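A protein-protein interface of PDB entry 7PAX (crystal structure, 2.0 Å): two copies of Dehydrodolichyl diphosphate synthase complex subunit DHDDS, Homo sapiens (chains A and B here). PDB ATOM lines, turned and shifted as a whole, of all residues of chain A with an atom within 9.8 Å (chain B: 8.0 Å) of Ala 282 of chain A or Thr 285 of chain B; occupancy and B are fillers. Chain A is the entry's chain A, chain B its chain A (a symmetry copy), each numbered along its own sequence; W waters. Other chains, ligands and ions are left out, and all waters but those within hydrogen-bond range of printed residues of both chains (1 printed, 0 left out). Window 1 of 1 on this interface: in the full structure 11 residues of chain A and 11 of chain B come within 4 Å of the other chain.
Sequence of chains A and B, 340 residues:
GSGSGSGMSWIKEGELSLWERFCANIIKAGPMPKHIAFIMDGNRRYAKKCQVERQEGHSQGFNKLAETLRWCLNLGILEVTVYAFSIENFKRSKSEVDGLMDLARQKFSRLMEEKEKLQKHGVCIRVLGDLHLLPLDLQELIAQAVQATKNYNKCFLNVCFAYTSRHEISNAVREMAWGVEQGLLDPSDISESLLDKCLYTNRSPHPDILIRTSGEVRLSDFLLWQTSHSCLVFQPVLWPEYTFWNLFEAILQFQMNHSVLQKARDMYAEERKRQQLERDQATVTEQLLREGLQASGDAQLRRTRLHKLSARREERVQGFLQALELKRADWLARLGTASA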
ATOM      1  N   ARG A 274       5.392 -15.770  -4.623  1.00  0.00           N
ATOM      2  CA  ARG A 274       5.515 -17.064  -3.935  1.00  0.00           C
ATOM      3  C   ARG A 274       4.509 -18.075  -4.374  1.00  0.00           C
ATOM      4  O   ARG A 274       4.813 -19.192  -4.536  1.00  0.00           O
ATOM      5  CB  ARG A 274       5.393 -16.950  -2.427  1.00  0.00           C
ATOM      6  CG  ARG A 274       5.015 -18.260  -1.784  1.00  0.00           C
ATOM      7  CD  ARG A 274       4.907 -18.208  -0.290  1.00  0.00           C
ATOM      8  N   GLN A 275       3.276 -17.689  -4.467  1.00  0.00           N
ATOM      9  CA  GLN A 275       2.290 -18.623  -5.019  1.00  0.00           C
ATOM     10  C   GLN A 275       2.611 -18.981  -6.468  1.00  0.00           C
ATOM     11  O   GLN A 275       2.326 -20.099  -6.918  1.00  0.00           O
ATOM     12  CB  GLN A 275       0.873 -18.042  -4.927  1.00  0.00           C
ATOM     13  CG  GLN A 275       0.351 -17.874  -3.506  1.00  0.00           C
ATOM     14  CD  GLN A 275      -1.124 -17.496  -3.451  1.00  0.00           C
ATOM     15  OE1 GLN A 275      -1.881 -17.742  -4.390  1.00  0.00           O
ATOM     16  NE2 GLN A 275      -1.533 -16.882  -2.347  1.00  0.00           N
ATOM     17  N   GLN A 276       3.187 -18.035  -7.214  1.00  0.00           N
ATOM     18  CA  GLN A 276       3.644 -18.317  -8.570  1.00  0.00           C
ATOM     19  C   GLN A 276       4.768 -19.344  -8.568  1.00  0.00           C
ATOM     20  O   GLN A 276       4.807 -20.238  -9.422  1.00  0.00           O
ATOM     21  CB  GLN A 276       4.107 -17.023  -9.237  1.00  0.00           C
ATOM     22  CG  GLN A 276       4.502 -17.174 -10.693  1.00  0.00           C
ATOM     23  CD  GLN A 276       3.328 -17.529 -11.574  1.00  0.00           C
ATOM     24  OE1 GLN A 276       3.250 -18.638 -12.104  1.00  0.00           O
ATOM     25  NE2 GLN A 276       2.403 -16.590 -11.737  1.00  0.00           N
ATOM     26  N   LEU A 277       5.695 -19.229  -7.613  1.00  0.00           N
ATOM     27  CA  LEU A 277       6.781 -20.196  -7.517  1.00  0.00           C
ATOM     28  C   LEU A 277       6.246 -21.592  -7.230  1.00  0.00           C
ATOM     29  O   LEU A 277       6.741 -22.583  -7.778  1.00  0.00           O
ATOM     30  CB  LEU A 277       7.772 -19.767  -6.435  1.00  0.00           C
ATOM     31  CG  LEU A 277       8.973 -20.695  -6.230  1.00  0.00           C
ATOM     32  CD1 LEU A 277       9.713 -20.921  -7.543  1.00  0.00           C
ATOM     33  CD2 LEU A 277       9.910 -20.150  -5.163  1.00  0.00           C
ATOM     34  N   GLU A 278       5.222 -21.688  -6.382  1.00  0.00           N
ATOM     35  CA  GLU A 278       4.686 -22.996  -6.022  1.00  0.00           C
ATOM     36  C   GLU A 278       3.922 -23.619  -7.184  1.00  0.00           C
ATOM     37  O   GLU A 278       4.008 -24.832  -7.407  1.00  0.00           O
ATOM     38  CB  GLU A 278       3.801 -22.860  -4.786  1.00  0.00           C
ATOM     39  CG  GLU A 278       4.583 -22.447  -3.550  1.00  0.00           C
ATOM     40  CD  GLU A 278       3.727 -22.352  -2.304  1.00  0.00           C
ATOM     41  OE1 GLU A 278       2.522 -22.054  -2.428  1.00  0.00           O
ATOM     42  OE2 GLU A 278       4.263 -22.570  -1.198  1.00  0.00           O
ATOM     43  N   ARG A 279       3.170 -22.807  -7.934  1.00  0.00           N
ATOM     44  CA  ARG A 279       2.516 -23.314  -9.136  1.00  0.00           C
ATOM     45  C   ARG A 279       3.546 -23.814 -10.142  1.00  0.00           C
ATOM     46  O   ARG A 279       3.363 -24.870 -10.759  1.00  0.00           O
ATOM     47  CB  ARG A 279       1.635 -22.230  -9.762  1.00  0.00           C
ATOM     48  CG  ARG A 279       0.415 -21.841  -8.934  1.00  0.00           C
ATOM     49  N   ASP A 280       4.647 -23.077 -10.300  1.00  0.00           N
ATOM     50  CA  ASP A 280       5.678 -23.481 -11.252  1.00  0.00           C
ATOM     51  C   ASP A 280       6.392 -24.742 -10.784  1.00  0.00           C
ATOM     52  O   ASP A 280       6.635 -25.660 -11.577  1.00  0.00           O
ATOM     53  CB  ASP A 280       6.674 -22.341 -11.460  1.00  0.00           C
ATOM     54  CG  ASP A 280       6.073 -21.183 -12.221  1.00  0.00           C
ATOM     55  OD1 ASP A 280       5.067 -21.401 -12.929  1.00  0.00           O
ATOM     56  OD2 ASP A 280       6.595 -20.054 -12.100  1.00  0.00           O
ATOM     57  N   GLN A 281       6.743 -24.804  -9.496  1.00  0.00           N
ATOM     58  CA  GLN A 281       7.346 -26.021  -8.965  1.00  0.00           C
ATOM     59  C   GLN A 281       6.409 -27.208  -9.136  1.00  0.00           C
ATOM     60  O   GLN A 281       6.848 -28.307  -9.492  1.00  0.00           O
ATOM     61  CB  GLN A 281       7.718 -25.833  -7.492  1.00  0.00           C
ATOM     62  CG  GLN A 281       8.825 -24.806  -7.242  1.00  0.00           C
ATOM     63  CD  GLN A 281      10.219 -25.365  -7.461  1.00  0.00           C
ATOM     64  OE1 GLN A 281      10.402 -26.361  -8.163  1.00  0.00           O
ATOM     65  NE2 GLN A 281      11.212 -24.728  -6.849  1.00  0.00           N
ATOM     66  N   ALA A 282       5.108 -26.998  -8.910  1.00  0.00           N
ATOM     67  CA  ALA A 282       4.145 -28.083  -9.082  1.00  0.00           C
ATOM     68  C   ALA A 282       4.066 -28.526 -10.539  1.00  0.00           C
ATOM     69  O   ALA A 282       3.956 -29.727 -10.821  1.00  0.00           O
ATOM     70  CB  ALA A 282       2.767 -27.654  -8.576  1.00  0.00           C
ATOM     71  N   THR A 283       4.124 -27.573 -11.475  1.00  0.00           N
ATOM     72  CA  THR A 283       4.099 -27.923 -12.892  1.00  0.00           C
ATOM     73  C   THR A 283       5.348 -28.706 -13.279  1.00  0.00           C
ATOM     74  O   THR A 283       5.266 -29.728 -13.973  1.00  0.00           O
ATOM     75  CB  THR A 283       3.967 -26.656 -13.742  1.00  0.00           C
ATOM     76  OG1 THR A 283       2.631 -26.150 -13.638  1.00  0.00           O
ATOM     77  CG2 THR A 283       4.271 -26.959 -15.206  1.00  0.00           C
ATOM     78  N   VAL A 284       6.516 -28.244 -12.827  1.00  0.00           N
ATOM     79  CA  VAL A 284       7.755 -28.977 -13.069  1.00  0.00           C
ATOM     80  C   VAL A 284       7.675 -30.370 -12.456  1.00  0.00           C
ATOM     81  O   VAL A 284       8.130 -31.355 -13.050  1.00  0.00           O
ATOM     82  CB  VAL A 284       8.958 -28.177 -12.527  1.00  0.00           C
ATOM     83  CG1 VAL A 284      10.207 -29.054 -12.468  1.00  0.00           C
ATOM     84  CG2 VAL A 284       9.196 -26.939 -13.377  1.00  0.00           C
ATOM     85  N   THR A 285       7.068 -30.476 -11.270  1.00  0.00           N
ATOM     86  CA  THR A 285       6.895 -31.784 -10.643  1.00  0.00           C
ATOM     87  C   THR A 285       6.002 -32.687 -11.486  1.00  0.00           C
ATOM     88  O   THR A 285       6.287 -33.881 -11.644  1.00  0.00           O
ATOM     89  CB  THR A 285       6.311 -31.620  -9.236  1.00  0.00           C
ATOM     90  OG1 THR A 285       7.285 -31.022  -8.372  1.00  0.00           O
ATOM     91  CG2 THR A 285       5.904 -32.974  -8.659  1.00  0.00           C
ATOM     92  N   GLU A 286       4.915 -32.134 -12.037  1.00  0.00           N
ATOM     93  CA  GLU A 286       4.012 -32.933 -12.862  1.00  0.00           C
ATOM     94  C   GLU A 286       4.720 -33.460 -14.104  1.00  0.00           C
ATOM     95  O   GLU A 286       4.556 -34.628 -14.474  1.00  0.00           O
ATOM     96  CB  GLU A 286       2.787 -32.106 -13.251  1.00  0.00           C
ATOM     97  N   GLN A 287       5.516 -32.612 -14.760  1.00  0.00           N
ATOM     98  CA  GLN A 287       6.331 -33.075 -15.874  1.00  0.00           C
ATOM     99  C   GLN A 287       7.378 -34.090 -15.433  1.00  0.00           C
ATOM    100  O   GLN A 287       7.815 -34.909 -16.248  1.00  0.00           O
ATOM    101  CB  GLN A 287       7.006 -31.887 -16.566  1.00  0.00           C
ATOM    102  N   LEU A 288       7.780 -34.067 -14.162  1.00  0.00           N
ATOM    103  CA  LEU A 288       8.734 -35.038 -13.642  1.00  0.00           C
ATOM    104  C   LEU A 288       8.072 -36.265 -13.029  1.00  0.00           C
ATOM    105  O   LEU A 288       8.704 -37.327 -12.985  1.00  0.00           O
ATOM    106  CB  LEU A 288       9.652 -34.378 -12.608  1.00  0.00           C
ATOM    107  CG  LEU A 288      10.633 -33.356 -13.184  1.00  0.00           C
ATOM    108  CD1 LEU A 288      11.804 -33.137 -12.244  1.00  0.00           C
ATOM    109  CD2 LEU A 288      11.122 -33.804 -14.555  1.00  0.00           C
ATOM    110  N   LEU A 289       6.834 -36.150 -12.544  1.00  0.00           N
ATOM    111  CA  LEU A 289       6.052 -37.346 -12.244  1.00  0.00           C
ATOM    112  C   LEU A 289       5.854 -38.174 -13.507  1.00  0.00           C
ATOM    113  O   LEU A 289       6.081 -39.389 -13.514  1.00  0.00           O
ATOM    114  CB  LEU A 289       4.707 -36.959 -11.625  1.00  0.00           C
ATOM    115  N   ARG A 290       5.441 -37.524 -14.593  1.00  0.00           N
ATOM    116  CA  ARG A 290       5.542 -38.129 -15.907  1.00  0.00           C
ATOM    117  C   ARG A 290       7.010 -38.184 -16.328  1.00  0.00           C
ATOM    118  O   ARG A 290       7.898 -37.654 -15.653  1.00  0.00           O
ATOM    119  CB  ARG A 290       4.710 -37.347 -16.924  1.00  0.00           C
ATOM    120  N   ALA A 295      11.788 -36.622  -8.402  1.00  0.00           N
ATOM    121  CA  ALA A 295      11.373 -35.302  -7.942  1.00  0.00           C
ATOM    122  C   ALA A 295      12.557 -34.438  -7.527  1.00  0.00           C
ATOM    123  O   ALA A 295      12.447 -33.207  -7.546  1.00  0.00           O
ATOM    124  CB  ALA A 295      10.394 -35.430  -6.774  1.00  0.00           C
ATOM    125  N   ARG A 302      15.170 -30.372 -11.636  1.00  0.00           N
ATOM    126  CA  ARG A 302      13.990 -29.520 -11.539  1.00  0.00           C
ATOM    127  C   ARG A 302      14.349 -28.040 -11.507  1.00  0.00           C
ATOM    128  O   ARG A 302      13.500 -27.196 -11.822  1.00  0.00           O
ATOM    129  CB  ARG A 302      13.169 -29.911 -10.308  1.00  0.00           C
ATOM    130  CG  ARG A 302      13.797 -29.545  -8.978  1.00  0.00           C
ATOM    131  CD  ARG A 302      12.839 -29.801  -7.814  1.00  0.00           C
ATOM    132  NE  ARG A 302      11.554 -29.138  -8.008  1.00  0.00           N
ATOM    133  CZ  ARG A 302      10.385 -29.768  -8.086  1.00  0.00           C
ATOM    134  NH1 ARG A 302      10.321 -31.088  -7.965  1.00  0.00           N
ATOM    135  NH2 ARG A 302       9.273 -29.071  -8.274  1.00  0.00           N
ATOM    136  N   LEU A 306      12.903 -25.469 -14.019  1.00  0.00           N
ATOM    137  CA  LEU A 306      12.280 -24.254 -13.498  1.00  0.00           C
ATOM    138  C   LEU A 306      12.877 -23.006 -14.139  1.00  0.00           C
ATOM    139  O   LEU A 306      12.148 -22.068 -14.485  1.00  0.00           O
ATOM    140  CB  LEU A 306      12.434 -24.201 -11.979  1.00  0.00           C
ATOM    141  CG  LEU A 306      11.583 -23.179 -11.227  1.00  0.00           C
ATOM    142  CD1 LEU A 306      10.108 -23.568 -11.275  1.00  0.00           C
ATOM    143  CD2 LEU A 306      12.064 -23.030  -9.789  1.00  0.00           C
ATOM    144  N   LEU A 309      11.557 -22.932 -17.741  1.00  0.00           N
ATOM    145  CA  LEU A 309      10.129 -22.631 -17.778  1.00  0.00           C
ATOM    146  C   LEU A 309       9.889 -21.126 -17.701  1.00  0.00           C
ATOM    147  O   LEU A 309       9.152 -20.558 -18.515  1.00  0.00           O
ATOM    148  CB  LEU A 309       9.408 -23.356 -16.637  1.00  0.00           C
ATOM    149  CG  LEU A 309       7.932 -23.023 -16.391  1.00  0.00           C
ATOM    150  CD1 LEU A 309       7.163 -24.279 -16.015  1.00  0.00           C
ATOM    151  CD2 LEU A 309       7.767 -21.970 -15.301  1.00  0.00           C
ATOM    152  N   GLU B 278      11.998 -30.679  -1.269  1.00  0.00           N
ATOM    153  CA  GLU B 278      11.372 -30.789  -2.581  1.00  0.00           C
ATOM    154  C   GLU B 278      10.569 -32.078  -2.705  1.00  0.00           C
ATOM    155  O   GLU B 278       9.485 -32.082  -3.300  1.00  0.00           O
ATOM    156  CB  GLU B 278      12.443 -30.698  -3.665  1.00  0.00           C
ATOM    157  CG  GLU B 278      13.116 -29.336  -3.708  1.00  0.00           C
ATOM    158  CD  GLU B 278      14.150 -29.214  -4.808  1.00  0.00           C
ATOM    159  OE1 GLU B 278      14.758 -30.240  -5.173  1.00  0.00           O
ATOM    160  OE2 GLU B 278      14.359 -28.088  -5.303  1.00  0.00           O
ATOM    161  N   ARG B 279      11.082 -33.181  -2.150  1.00  0.00           N
ATOM    162  CA  ARG B 279      10.307 -34.417  -2.120  1.00  0.00           C
ATOM    163  C   ARG B 279       9.021 -34.230  -1.324  1.00  0.00           C
ATOM    164  O   ARG B 279       7.952 -34.699  -1.732  1.00  0.00           O
ATOM    165  CB  ARG B 279      11.143 -35.557  -1.531  1.00  0.00           C
ATOM    166  CG  ARG B 279      12.321 -35.997  -2.394  1.00  0.00           C
ATOM    167  N   ASP B 280       9.103 -33.522  -0.195  1.00  0.00           N
ATOM    168  CA  ASP B 280       7.919 -33.305   0.631  1.00  0.00           C
ATOM    169  C   ASP B 280       6.926 -32.384  -0.066  1.00  0.00           C
ATOM    170  O   ASP B 280       5.717 -32.646  -0.065  1.00  0.00           O
ATOM    171  CB  ASP B 280       8.325 -32.735   1.989  1.00  0.00           C
ATOM    172  CG  ASP B 280       9.046 -33.748   2.847  1.00  0.00           C
ATOM    173  OD1 ASP B 280       8.879 -34.960   2.594  1.00  0.00           O
ATOM    174  OD2 ASP B 280       9.788 -33.334   3.764  1.00  0.00           O
ATOM    175  N   GLN B 281       7.418 -31.295  -0.663  1.00  0.00           N
ATOM    176  CA  GLN B 281       6.532 -30.422  -1.425  1.00  0.00           C
ATOM    177  C   GLN B 281       5.872 -31.184  -2.564  1.00  0.00           C
ATOM    178  O   GLN B 281       4.677 -31.007  -2.828  1.00  0.00           O
ATOM    179  CB  GLN B 281       7.305 -29.214  -1.960  1.00  0.00           C
ATOM    180  CG  GLN B 281       7.822 -28.261  -0.879  1.00  0.00           C
ATOM    181  CD  GLN B 281       6.764 -27.290  -0.383  1.00  0.00           C
ATOM    182  OE1 GLN B 281       5.564 -27.535  -0.516  1.00  0.00           O
ATOM    183  NE2 GLN B 281       7.210 -26.174   0.184  1.00  0.00           N
ATOM    184  N   ALA B 282       6.628 -32.058  -3.236  1.00  0.00           N
ATOM    185  CA  ALA B 282       6.055 -32.847  -4.324  1.00  0.00           C
ATOM    186  C   ALA B 282       4.986 -33.804  -3.808  1.00  0.00           C
ATOM    187  O   ALA B 282       3.953 -33.998  -4.464  1.00  0.00           O
ATOM    188  CB  ALA B 282       7.155 -33.616  -5.058  1.00  0.00           C
ATOM    189  N   THR B 283       5.215 -34.407  -2.637  1.00  0.00           N
ATOM    190  CA  THR B 283       4.219 -35.304  -2.057  1.00  0.00           C
ATOM    191  C   THR B 283       2.955 -34.539  -1.682  1.00  0.00           C
ATOM    192  O   THR B 283       1.836 -34.981  -1.973  1.00  0.00           O
ATOM    193  CB  THR B 283       4.804 -36.017  -0.836  1.00  0.00           C
ATOM    194  OG1 THR B 283       5.739 -37.012  -1.268  1.00  0.00           O
ATOM    195  CG2 THR B 283       3.699 -36.691  -0.029  1.00  0.00           C
ATOM    196  N   VAL B 284       3.118 -33.377  -1.044  1.00  0.00           N
ATOM    197  CA  VAL B 284       1.971 -32.532  -0.725  1.00  0.00           C
ATOM    198  C   VAL B 284       1.243 -32.124  -2.001  1.00  0.00           C
ATOM    199  O   VAL B 284       0.007 -32.091  -2.048  1.00  0.00           O
ATOM    200  CB  VAL B 284       2.428 -31.307   0.093  1.00  0.00           C
ATOM    201  CG1 VAL B 284       1.323 -30.254   0.152  1.00  0.00           C
ATOM    202  CG2 VAL B 284       2.855 -31.733   1.489  1.00  0.00           C
ATOM    203  N   THR B 285       2.000 -31.835  -3.065  1.00  0.00           N
ATOM    204  CA  THR B 285       1.378 -31.496  -4.343  1.00  0.00           C
ATOM    205  C   THR B 285       0.572 -32.667  -4.893  1.00  0.00           C
ATOM    206  O   THR B 285      -0.537 -32.477  -5.410  1.00  0.00           O
ATOM    207  CB  THR B 285       2.450 -31.066  -5.350  1.00  0.00           C
ATOM    208  OG1 THR B 285       3.002 -29.802  -4.963  1.00  0.00           O
ATOM    209  CG2 THR B 285       1.853 -30.936  -6.750  1.00  0.00           C
ATOM    210  N   GLU B 286       1.111 -33.887  -4.790  1.00  0.00           N
ATOM    211  CA  GLU B 286       0.398 -35.060  -5.291  1.00  0.00           C
ATOM    212  C   GLU B 286      -0.913 -35.269  -4.543  1.00  0.00           C
ATOM    213  O   GLU B 286      -1.946 -35.561  -5.155  1.00  0.00           O
ATOM    214  CB  GLU B 286       1.285 -36.300  -5.179  1.00  0.00           C
ATOM    215  N   GLN B 287      -0.891 -35.119  -3.217  1.00  0.00           N
ATOM    216  CA  GLN B 287      -2.126 -35.167  -2.447  1.00  0.00           C
ATOM    217  C   GLN B 287      -3.064 -34.021  -2.800  1.00  0.00           C
ATOM    218  O   GLN B 287      -4.280 -34.152  -2.623  1.00  0.00           O
ATOM    219  CB  GLN B 287      -1.815 -35.154  -0.947  1.00  0.00           C
ATOM    220  N   LEU B 288      -2.535 -32.908  -3.307  1.00  0.00           N
ATOM    221  CA  LEU B 288      -3.365 -31.785  -3.725  1.00  0.00           C
ATOM    222  C   LEU B 288      -3.751 -31.836  -5.197  1.00  0.00           C
ATOM    223  O   LEU B 288      -4.780 -31.259  -5.567  1.00  0.00           O
ATOM    224  CB  LEU B 288      -2.656 -30.461  -3.425  1.00  0.00           C
ATOM    225  CG  LEU B 288      -2.526 -30.127  -1.938  1.00  0.00           C
ATOM    226  CD1 LEU B 288      -2.299 -28.641  -1.732  1.00  0.00           C
ATOM    227  CD2 LEU B 288      -3.762 -30.591  -1.180  1.00  0.00           C
ATOM    228  N   LEU B 289      -2.956 -32.492  -6.046  1.00  0.00           N
ATOM    229  CA  LEU B 289      -3.436 -32.836  -7.381  1.00  0.00           C
ATOM    230  C   LEU B 289      -4.658 -33.740  -7.281  1.00  0.00           C
ATOM    231  O   LEU B 289      -5.684 -33.499  -7.929  1.00  0.00           O
ATOM    232  CB  LEU B 289      -2.323 -33.505  -8.190  1.00  0.00           C
ATOM    233  N   ARG B 290      -4.568 -34.784  -6.460  1.00  0.00           N
ATOM    234  CA  ARG B 290      -5.755 -35.503  -6.036  1.00  0.00           C
ATOM    235  C   ARG B 290      -6.555 -34.633  -5.067  1.00  0.00           C
ATOM    236  O   ARG B 290      -6.121 -33.551  -4.659  1.00  0.00           O
ATOM    237  CB  ARG B 290      -5.373 -36.834  -5.389  1.00  0.00           C
ATOM    238  N   GLU B 291      -7.751 -35.110  -4.713  1.00  0.00           N
ATOM    239  CA  GLU B 291      -8.702 -34.361  -3.892  1.00  0.00           C
ATOM    240  C   GLU B 291      -9.185 -33.091  -4.592  1.00  0.00           C
ATOM    241  O   GLU B 291     -10.113 -32.433  -4.113  1.00  0.00           O
ATOM    242  CB  GLU B 291      -8.107 -34.011  -2.519  1.00  0.00           C
ATOM    243  CG  GLU B 291      -7.368 -35.151  -1.825  1.00  0.00           C
ATOM    244  CD  GLU B 291      -6.486 -34.669  -0.680  1.00  0.00           C
ATOM    245  OE1 GLU B 291      -6.462 -33.447  -0.416  1.00  0.00           O
ATOM    246  OE2 GLU B 291      -5.816 -35.512  -0.045  1.00  0.00           O
ATOM    247  N   LEU B 293      -8.003 -30.101  -4.951  1.00  0.00           N
ATOM    248  CA  LEU B 293      -7.689 -28.779  -4.431  1.00  0.00           C
ATOM    249  C   LEU B 293      -6.589 -28.118  -5.268  1.00  0.00           C
ATOM    250  O   LEU B 293      -5.988 -28.730  -6.155  1.00  0.00           O
ATOM    251  CB  LEU B 293      -7.273 -28.867  -2.962  1.00  0.00           C
ATOM    252  N   GLN B 294      -6.329 -26.847  -4.970  1.00  0.00           N
ATOM    253  CA  GLN B 294      -5.376 -26.061  -5.740  1.00  0.00           C
ATOM    254  C   GLN B 294      -3.946 -26.306  -5.263  1.00  0.00           C
ATOM    255  O   GLN B 294      -3.700 -26.736  -4.133  1.00  0.00           O
ATOM    256  CB  GLN B 294      -5.708 -24.570  -5.643  1.00  0.00           C
ATOM    257  CG  GLN B 294      -6.929 -24.146  -6.440  1.00  0.00           C
ATOM    258  CD  GLN B 294      -6.813 -24.503  -7.909  1.00  0.00           C
ATOM    259  OE1 GLN B 294      -5.798 -24.230  -8.549  1.00  0.00           O
ATOM    260  NE2 GLN B 294      -7.857 -25.119  -8.450  1.00  0.00           N
ATOM    261  N   ALA B 295      -2.990 -26.018  -6.153  1.00  0.00           N
ATOM    262  CA  ALA B 295      -1.580 -26.124  -5.797  1.00  0.00           C
ATOM    263  C   ALA B 295      -1.132 -24.998  -4.875  1.00  0.00           C
ATOM    264  O   ALA B 295      -0.151 -25.167  -4.142  1.00  0.00           O
ATOM    265  CB  ALA B 295      -0.712 -26.134  -7.058  1.00  0.00           C
ATOM    266  N   SER B 296      -1.824 -23.861  -4.901  1.00  0.00           N
ATOM    267  CA  SER B 296      -1.512 -22.724  -4.046  1.00  0.00           C
ATOM    268  C   SER B 296      -2.751 -21.857  -3.899  1.00  0.00           C
ATOM    269  O   SER B 296      -3.646 -21.875  -4.748  1.00  0.00           O
ATOM    270  CB  SER B 296      -0.353 -21.892  -4.602  1.00  0.00           C
ATOM    271  OG  SER B 296       0.872 -22.310  -4.040  1.00  0.00           O
ATOM    272  N   ARG B 302      -1.084 -25.819   1.415  1.00  0.00           N
ATOM    273  CA  ARG B 302       0.057 -26.718   1.286  1.00  0.00           C
ATOM    274  C   ARG B 302       1.084 -26.507   2.392  1.00  0.00           C
ATOM    275  O   ARG B 302       1.884 -27.411   2.666  1.00  0.00           O
ATOM    276  CB  ARG B 302       0.695 -26.550  -0.094  1.00  0.00           C
ATOM    277  CG  ARG B 302       1.437 -25.244  -0.301  1.00  0.00           C
ATOM    278  CD  ARG B 302       2.195 -25.233  -1.629  1.00  0.00           C
ATOM    279  NE  ARG B 302       3.078 -26.387  -1.765  1.00  0.00           N
ATOM    280  CZ  ARG B 302       2.981 -27.301  -2.725  1.00  0.00           C
ATOM    281  NH1 ARG B 302       2.048 -27.197  -3.663  1.00  0.00           N
ATOM    282  NH2 ARG B 302       3.829 -28.319  -2.753  1.00  0.00           N
ATOM    283  N   ARG B 305      -0.289 -28.505   5.398  1.00  0.00           N
ATOM    284  CA  ARG B 305      -0.066 -29.904   5.044  1.00  0.00           C
ATOM    285  C   ARG B 305       1.413 -30.265   5.151  1.00  0.00           C
ATOM    286  O   ARG B 305       1.762 -31.351   5.627  1.00  0.00           O
ATOM    287  CB  ARG B 305      -0.586 -30.179   3.634  1.00  0.00           C
ATOM    288  N   LEU B 306       2.296 -29.363   4.712  1.00  0.00           N
ATOM    289  CA  LEU B 306       3.733 -29.585   4.858  1.00  0.00           C
ATOM    290  C   LEU B 306       4.145 -29.603   6.326  1.00  0.00           C
ATOM    291  O   LEU B 306       4.957 -30.439   6.740  1.00  0.00           O
ATOM    292  CB  LEU B 306       4.506 -28.508   4.098  1.00  0.00           C
ATOM    293  CG  LEU B 306       5.998 -28.749   3.872  1.00  0.00           C
ATOM    294  CD1 LEU B 306       6.214 -29.895   2.888  1.00  0.00           C
ATOM    295  CD2 LEU B 306       6.682 -27.476   3.389  1.00  0.00           C
ATOM    296  N   LEU B 309       2.818 -32.906   7.757  1.00  0.00           N
ATOM    297  CA  LEU B 309       3.555 -34.050   7.228  1.00  0.00           C
ATOM    298  C   LEU B 309       4.845 -34.274   8.012  1.00  0.00           C
ATOM    299  O   LEU B 309       5.132 -35.391   8.457  1.00  0.00           O
ATOM    300  CB  LEU B 309       3.852 -33.842   5.740  1.00  0.00           C
ATOM    301  CG  LEU B 309       4.779 -34.844   5.043  1.00  0.00           C
ATOM    302  CD1 LEU B 309       4.287 -35.127   3.634  1.00  0.00           C
ATOM    303  CD2 LEU B 309       6.218 -34.344   4.998  1.00  0.00           C
HETATM  304  O   HOH W   1       5.929 -29.455  -6.024  1.00  0.00           O
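Of the 21 printed residues of chain A, 5 touch a printed residue of chain B. Along chain A the printed residues that touch a printed residue of chain B span positions 275 to 302. Along chain B the printed residues that touch a printed residue of chain A span positions 278 to 302. Among the printed residues, no Asp or Glu carboxylate lies within 4 Å of a Lys or Arg side-chain nitrogen of the other chain.
Glu 278 of chain A touches Arg 302 of chain B, and with the chains exchanged Arg 302 of chain A touches Glu 278 of chain B. Ala 282 of chain A touches Thr 285 of chain B, and with the chains exchanged Thr 285 of chain A touches Ala 282 of chain B. Of the 6 pairs that touch across the chains among the printed residues, 4 have their exchanged pair printed and touching as well.
The backbone carbonyl oxygen (O) of Ala 295 of chain B sits at hydrogen-bond distance from the guanidinium group (NH1) of Arg 302 of chain B (3.0 Å). The backbone carbonyl oxygen (O) of Gln 281 of chain A lies within hydrogen-bond range of the guanidinium group (NH2) of Arg 302 of chain A (2.8 Å). The backbone carbonyl oxygen (O) of Gln 281 of chain B sits at hydrogen-bond distance from the side-chain hydroxyl (OG1) of Thr 285 of chain B.
OE1 of Glu 278 of chain A lies close to OG of Ser 296 of chain B.
Among the printed residues, merely in contact across the chains: Gln 275 of chain A with Ser 296 of chain B, Glu 278 of chain A with Arg 302 of chain B, Ala 282 of chain A with Thr 285 of chain B, Thr 285 of chain A with Ala 282 of chain B and Arg 302 of chain A with Glu 278 of chain B.
Of the printed residues of chain B, Glu 278 of chain A touches Ser 296 (2.3 Å) and Arg 302 (3.3 Å). Printed residues of chain B within 4 Å of Thr 285 of chain A: Ala 282 (3.9 Å). Leu 289 of chain A touches none of the printed residues of chain B. Of the printed residues of chain A, Glu 278 of chain B touches Arg 302 (3.3 Å). Printed residues of chain A within 4 Å of Ala 282 of chain B: Thr 285. No residue of chain A comes within 4 Å of Gln 287 of chain B. Of the printed residues of chain A, Ser 296 of chain B touches Gln 275 (3.9 Å) and Glu 278 (2.3 Å). Of the printed residues of chain A, Arg 302 of chain B touches Glu 278. The nearest residue of chain A that does not touch Thr 285 of chain B is Thr 285 of chain A (4.9 Å). The nearest printed residue of chain B that does not touch Thr 285 of chain A is Thr 285 of chain B (4.9 Å).
Water W1 bridges the side-chain hydroxyl of Thr 285 of chain A (3.1 Å) and the side-chain hydroxyl of Thr 285 of chain B (3.1 Å).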
